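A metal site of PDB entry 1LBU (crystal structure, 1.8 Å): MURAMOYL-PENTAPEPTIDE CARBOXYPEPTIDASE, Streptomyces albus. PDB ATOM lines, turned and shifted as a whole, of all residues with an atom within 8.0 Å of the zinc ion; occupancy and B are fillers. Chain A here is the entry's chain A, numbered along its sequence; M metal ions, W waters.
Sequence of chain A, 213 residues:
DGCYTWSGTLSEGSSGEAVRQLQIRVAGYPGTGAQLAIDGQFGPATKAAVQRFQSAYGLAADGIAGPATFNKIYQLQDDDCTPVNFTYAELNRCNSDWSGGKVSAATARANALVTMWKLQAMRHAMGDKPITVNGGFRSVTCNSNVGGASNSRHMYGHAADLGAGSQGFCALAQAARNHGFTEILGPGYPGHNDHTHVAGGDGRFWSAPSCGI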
ATOM      1  N   GLY A 135     -20.787  -5.511   7.166  1.00  0.00           N
ATOM      2  CA  GLY A 135     -19.394  -5.750   7.648  1.00  0.00           C
ATOM      3  C   GLY A 135     -19.107  -4.608   8.665  1.00  0.00           C
ATOM      4  O   GLY A 135     -19.887  -3.678   8.734  1.00  0.00           O
ATOM      5  N   GLY A 136     -18.035  -4.797   9.405  1.00  0.00           N
ATOM      6  CA  GLY A 136     -17.593  -3.859  10.420  1.00  0.00           C
ATOM      7  C   GLY A 136     -16.090  -3.877  10.636  1.00  0.00           C
ATOM      8  O   GLY A 136     -15.287  -3.175  10.013  1.00  0.00           O
ATOM      9  N   ARG A 138     -12.438  -5.426  10.555  1.00  0.00           N
ATOM     10  CA  ARG A 138     -11.573  -6.128   9.640  1.00  0.00           C
ATOM     11  C   ARG A 138     -10.140  -6.105  10.209  1.00  0.00           C
ATOM     12  O   ARG A 138      -9.532  -5.035  10.462  1.00  0.00           O
ATOM     13  CB  ARG A 138     -11.620  -5.622   8.188  1.00  0.00           C
ATOM     14  CG  ARG A 138     -13.060  -5.596   7.631  1.00  0.00           C
ATOM     15  CD  ARG A 138     -13.208  -5.483   6.155  1.00  0.00           C
ATOM     16  NE  ARG A 138     -12.506  -4.344   5.619  1.00  0.00           N
ATOM     17  CZ  ARG A 138     -12.935  -3.396   4.810  1.00  0.00           C
ATOM     18  NH1 ARG A 138     -14.212  -3.297   4.390  1.00  0.00           N
ATOM     19  NH2 ARG A 138     -12.052  -2.477   4.384  1.00  0.00           N
ATOM     20  N   ASN A 143      -8.822  -7.249   5.700  1.00  0.00           N
ATOM     21  CA  ASN A 143      -8.788  -5.997   4.936  1.00  0.00           C
ATOM     22  C   ASN A 143      -8.110  -6.184   3.594  1.00  0.00           C
ATOM     23  O   ASN A 143      -8.577  -5.607   2.580  1.00  0.00           O
ATOM     24  CB  ASN A 143      -8.303  -4.786   5.779  1.00  0.00           C
ATOM     25  CG  ASN A 143      -8.382  -3.486   5.019  1.00  0.00           C
ATOM     26  OD1 ASN A 143      -9.478  -2.988   4.689  1.00  0.00           O
ATOM     27  ND2 ASN A 143      -7.238  -2.886   4.765  1.00  0.00           N
ATOM     28  N   VAL A 146     -10.021  -8.263   1.081  1.00  0.00           N
ATOM     29  CA  VAL A 146     -11.045  -7.443   0.425  1.00  0.00           C
ATOM     30  C   VAL A 146     -10.434  -6.447  -0.572  1.00  0.00           C
ATOM     31  O   VAL A 146     -11.130  -5.974  -1.471  1.00  0.00           O
ATOM     32  CB  VAL A 146     -11.947  -6.741   1.474  1.00  0.00           C
ATOM     33  CG1 VAL A 146     -11.615  -5.268   1.695  1.00  0.00           C
ATOM     34  CG2 VAL A 146     -13.434  -6.906   1.128  1.00  0.00           C
ATOM     35  N   SER A 152      -7.660   2.346   6.030  1.00  0.00           N
ATOM     36  CA  SER A 152      -8.997   1.918   6.394  1.00  0.00           C
ATOM     37  C   SER A 152      -9.330   1.972   7.869  1.00  0.00           C
ATOM     38  O   SER A 152      -8.664   1.345   8.731  1.00  0.00           O
ATOM     39  CB  SER A 152      -9.270   0.472   5.875  1.00  0.00           C
ATOM     40  OG  SER A 152     -10.678   0.229   6.064  1.00  0.00           O
ATOM     41  N   ARG A 153     -10.412   2.690   8.172  1.00  0.00           N
ATOM     42  CA  ARG A 153     -10.854   2.836   9.573  1.00  0.00           C
ATOM     43  C   ARG A 153     -11.525   1.545  10.015  1.00  0.00           C
ATOM     44  O   ARG A 153     -11.799   1.398  11.216  1.00  0.00           O
ATOM     45  CB  ARG A 153     -11.726   4.056   9.792  1.00  0.00           C
ATOM     46  CG  ARG A 153     -11.331   5.305   9.033  1.00  0.00           C
ATOM     47  CD  ARG A 153     -12.181   6.450   9.448  1.00  0.00           C
ATOM     48  NE  ARG A 153     -11.584   7.752   9.102  1.00  0.00           N
ATOM     49  CZ  ARG A 153     -12.099   8.943   9.249  1.00  0.00           C
ATOM     50  NH1 ARG A 153     -13.291   9.140   9.822  1.00  0.00           N
ATOM     51  NH2 ARG A 153     -11.470  10.051   8.834  1.00  0.00           N
ATOM     52  N   HIS A 154     -11.764   0.616   9.105  1.00  0.00           N
ATOM     53  CA  HIS A 154     -12.404  -0.677   9.434  1.00  0.00           C
ATOM     54  C   HIS A 154     -11.535  -1.449  10.430  1.00  0.00           C
ATOM     55  O   HIS A 154     -12.053  -2.186  11.267  1.00  0.00           O
ATOM     56  CB  HIS A 154     -12.601  -1.616   8.210  1.00  0.00           C
ATOM     57  CG  HIS A 154     -13.890  -1.288   7.500  1.00  0.00           C
ATOM     58  ND1 HIS A 154     -15.135  -1.821   7.867  1.00  0.00           N
ATOM     59  CD2 HIS A 154     -14.109  -0.437   6.471  1.00  0.00           C
ATOM     60  CE1 HIS A 154     -16.033  -1.307   7.040  1.00  0.00           C
ATOM     61  NE2 HIS A 154     -15.438  -0.478   6.187  1.00  0.00           N
ATOM     62  N   ALA A 159     -15.589   1.817  11.603  1.00  0.00           N
ATOM     63  CA  ALA A 159     -16.566   1.774  10.453  1.00  0.00           C
ATOM     64  C   ALA A 159     -17.485   0.592  10.371  1.00  0.00           C
ATOM     65  O   ALA A 159     -17.259  -0.483  10.910  1.00  0.00           O
ATOM     66  CB  ALA A 159     -15.636   1.755   9.191  1.00  0.00           C
ATOM     67  N   ALA A 160     -18.552   0.740   9.569  1.00  0.00           N
ATOM     68  CA  ALA A 160     -19.551  -0.293   9.272  1.00  0.00           C
ATOM     69  C   ALA A 160     -19.968  -0.081   7.798  1.00  0.00           C
ATOM     70  O   ALA A 160     -20.080   1.077   7.427  1.00  0.00           O
ATOM     71  CB  ALA A 160     -20.833  -0.155  10.075  1.00  0.00           C
ATOM     72  N   ASP A 161     -20.177  -1.169   7.112  1.00  0.00           N
ATOM     73  CA  ASP A 161     -20.663  -1.089   5.690  1.00  0.00           C
ATOM     74  C   ASP A 161     -22.161  -1.512   5.765  1.00  0.00           C
ATOM     75  O   ASP A 161     -22.475  -2.603   6.263  1.00  0.00           O
ATOM     76  CB  ASP A 161     -19.874  -2.091   4.836  1.00  0.00           C
ATOM     77  CG  ASP A 161     -18.462  -1.560   4.550  1.00  0.00           C
ATOM     78  OD1 ASP A 161     -18.297  -0.322   4.546  1.00  0.00           O
ATOM     79  OD2 ASP A 161     -17.603  -2.435   4.327  1.00  0.00           O
ATOM     80  N   LEU A 162     -23.016  -0.660   5.249  1.00  0.00           N
ATOM     81  CA  LEU A 162     -24.459  -0.831   5.284  1.00  0.00           C
ATOM     82  C   LEU A 162     -25.076  -1.286   3.961  1.00  0.00           C
ATOM     83  O   LEU A 162     -24.658  -0.705   2.944  1.00  0.00           O
ATOM     84  CB  LEU A 162     -25.061   0.549   5.699  1.00  0.00           C
ATOM     85  CG  LEU A 162     -25.097   0.974   7.136  1.00  0.00           C
ATOM     86  CD1 LEU A 162     -23.990   0.577   8.052  1.00  0.00           C
ATOM     87  CD2 LEU A 162     -25.310   2.497   7.358  1.00  0.00           C
ATOM     88  N   GLU A 183     -16.670  10.111   8.384  1.00  0.00           N
ATOM     89  CA  GLU A 183     -16.316   9.529   7.104  1.00  0.00           C
ATOM     90  C   GLU A 183     -17.547   8.843   6.493  1.00  0.00           C
ATOM     91  O   GLU A 183     -18.011   7.851   7.121  1.00  0.00           O
ATOM     92  CB  GLU A 183     -15.225   8.499   7.185  1.00  0.00           C
ATOM     93  CG  GLU A 183     -14.813   8.004   5.766  1.00  0.00           C
ATOM     94  CD  GLU A 183     -13.518   7.266   5.799  1.00  0.00           C
ATOM     95  OE1 GLU A 183     -13.661   6.158   6.326  1.00  0.00           O
ATOM     96  OE2 GLU A 183     -12.487   7.718   5.381  1.00  0.00           O
ATOM     97  N   LEU A 185     -18.934   7.232   2.796  1.00  0.00           N
ATOM     98  CA  LEU A 185     -18.643   7.050   1.330  1.00  0.00           C
ATOM     99  C   LEU A 185     -19.817   6.257   0.744  1.00  0.00           C
ATOM    100  O   LEU A 185     -20.238   5.261   1.379  1.00  0.00           O
ATOM    101  CB  LEU A 185     -17.310   6.324   1.267  1.00  0.00           C
ATOM    102  CG  LEU A 185     -16.069   7.027   1.775  1.00  0.00           C
ATOM    103  CD1 LEU A 185     -14.853   6.099   1.799  1.00  0.00           C
ATOM    104  CD2 LEU A 185     -15.702   8.240   0.878  1.00  0.00           C
ATOM    105  N   GLY A 191     -15.806   2.467  -6.006  1.00  0.00           N
ATOM    106  CA  GLY A 191     -15.948   1.213  -5.282  1.00  0.00           C
ATOM    107  C   GLY A 191     -16.975   1.263  -4.167  1.00  0.00           C
ATOM    108  O   GLY A 191     -16.976   0.382  -3.297  1.00  0.00           O
ATOM    109  N   HIS A 192     -17.860   2.231  -4.208  1.00  0.00           N
ATOM    110  CA  HIS A 192     -18.884   2.406  -3.178  1.00  0.00           C
ATOM    111  C   HIS A 192     -20.273   2.541  -3.720  1.00  0.00           C
ATOM    112  O   HIS A 192     -21.102   3.272  -3.123  1.00  0.00           O
ATOM    113  CB  HIS A 192     -18.542   3.591  -2.220  1.00  0.00           C
ATOM    114  CG  HIS A 192     -17.399   3.277  -1.299  1.00  0.00           C
ATOM    115  ND1 HIS A 192     -16.083   3.511  -1.632  1.00  0.00           N
ATOM    116  CD2 HIS A 192     -17.391   2.707  -0.075  1.00  0.00           C
ATOM    117  CE1 HIS A 192     -15.304   3.122  -0.631  1.00  0.00           C
ATOM    118  NE2 HIS A 192     -16.058   2.620   0.315  1.00  0.00           N
ATOM    119  N   HIS A 195     -23.070  -0.189  -1.475  1.00  0.00           N
ATOM    120  CA  HIS A 195     -23.084  -0.193   0.025  1.00  0.00           C
ATOM    121  C   HIS A 195     -22.766   1.241   0.416  1.00  0.00           C
ATOM    122  O   HIS A 195     -22.212   1.955  -0.390  1.00  0.00           O
ATOM    123  CB  HIS A 195     -22.162  -1.172   0.778  1.00  0.00           C
ATOM    124  CG  HIS A 195     -20.672  -0.884   0.673  1.00  0.00           C
ATOM    125  ND1 HIS A 195     -19.852  -1.380  -0.310  1.00  0.00           N
ATOM    126  CD2 HIS A 195     -19.845  -0.106   1.443  1.00  0.00           C
ATOM    127  CE1 HIS A 195     -18.613  -0.909  -0.142  1.00  0.00           C
ATOM    128  NE2 HIS A 195     -18.565  -0.128   0.927  1.00  0.00           N
ATOM    129  N   THR A 196     -23.166   1.490   1.642  1.00  0.00           N
ATOM    130  CA  THR A 196     -22.886   2.869   2.152  1.00  0.00           C
ATOM    131  C   THR A 196     -21.875   2.625   3.299  1.00  0.00           C
ATOM    132  O   THR A 196     -22.264   1.820   4.176  1.00  0.00           O
ATOM    133  CB  THR A 196     -24.108   3.633   2.648  1.00  0.00           C
ATOM    134  OG1 THR A 196     -25.005   3.984   1.535  1.00  0.00           O
ATOM    135  CG2 THR A 196     -23.648   4.941   3.404  1.00  0.00           C
ATOM    136  N   HIS A 197     -20.736   3.273   3.244  1.00  0.00           N
ATOM    137  CA  HIS A 197     -19.681   3.158   4.262  1.00  0.00           C
ATOM    138  C   HIS A 197     -19.848   4.343   5.241  1.00  0.00           C
ATOM    139  O   HIS A 197     -19.841   5.525   4.831  1.00  0.00           O
ATOM    140  CB  HIS A 197     -18.302   3.384   3.559  1.00  0.00           C
ATOM    141  CG  HIS A 197     -17.101   3.534   4.484  1.00  0.00           C
ATOM    142  ND1 HIS A 197     -16.320   2.486   4.923  1.00  0.00           N
ATOM    143  CD2 HIS A 197     -16.593   4.649   5.049  1.00  0.00           C
ATOM    144  CE1 HIS A 197     -15.356   3.048   5.763  1.00  0.00           C
ATOM    145  NE2 HIS A 197     -15.505   4.332   5.827  1.00  0.00           N
ATOM    146  N   VAL A 198     -19.948   4.000   6.554  1.00  0.00           N
ATOM    147  CA  VAL A 198     -20.029   5.084   7.582  1.00  0.00           C
ATOM    148  C   VAL A 198     -18.903   4.794   8.603  1.00  0.00           C
ATOM    149  O   VAL A 198     -18.699   3.599   8.965  1.00  0.00           O
ATOM    150  CB  VAL A 198     -21.440   5.126   8.179  1.00  0.00           C
ATOM    151  CG1 VAL A 198     -22.456   5.436   7.075  1.00  0.00           C
ATOM    152  CG2 VAL A 198     -21.939   3.917   8.973  1.00  0.00           C
ATOM    153  N   ALA A 199     -18.208   5.862   9.072  1.00  0.00           N
ATOM    154  CA  ALA A 199     -17.153   5.615  10.072  1.00  0.00           C
ATOM    155  C   ALA A 199     -16.991   6.840  10.968  1.00  0.00           C
ATOM    156  O   ALA A 199     -17.170   7.979  10.524  1.00  0.00           O
ATOM    157  CB  ALA A 199     -15.808   5.225   9.437  1.00  0.00           C
HETATM  158 ZN    ZN M   1     -16.443   0.382   4.488  1.00  0.00          ZN
HETATM  159  O   HOH W   1     -15.556   0.437   2.566  1.00  0.00           O
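Water W1 bridges a ring nitrogen (NE2) of His 192 (3.2 Å) and a ring nitrogen (NE2) of His 195 (3.5 Å).
Three residues have an atom within 4 Å of the zinc ion: His 154, Asp 161 and His 197.
The zinc ion is bound by the side-chain carboxylate of Asp 161 (2.0 Å), water W1 (2.1 Å), a ring nitrogen (ND1) of His 197 (2.2 Å) and a ring nitrogen (NE2) of His 154 (2.2 Å). The zinc ion has four donor atoms within binding distance.
The side-chain carboxylate of Asp 161 lies within salt-bridge range of the guanidinium group of Arg 138. N of Asp 161 is in hydrogen-bond range of O of Gly 135 (3.0 Å). N of His 197 lies within hydrogen-bond range of O of Leu 185. OE1 of Glu 183 sits at hydrogen-bond distance from NE2 of His 197 (2.6 Å). O of His 154 sits at hydrogen-bond distance from N of Arg 138 (3.3 Å). N of His 154 sits close to OG of Ser 152 (3.3 Å). A ring nitrogen (ND1) of His 154 lies within hydrogen-bond range of the backbone carbonyl oxygen (O) of Gly 136, at 2.5 Å.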
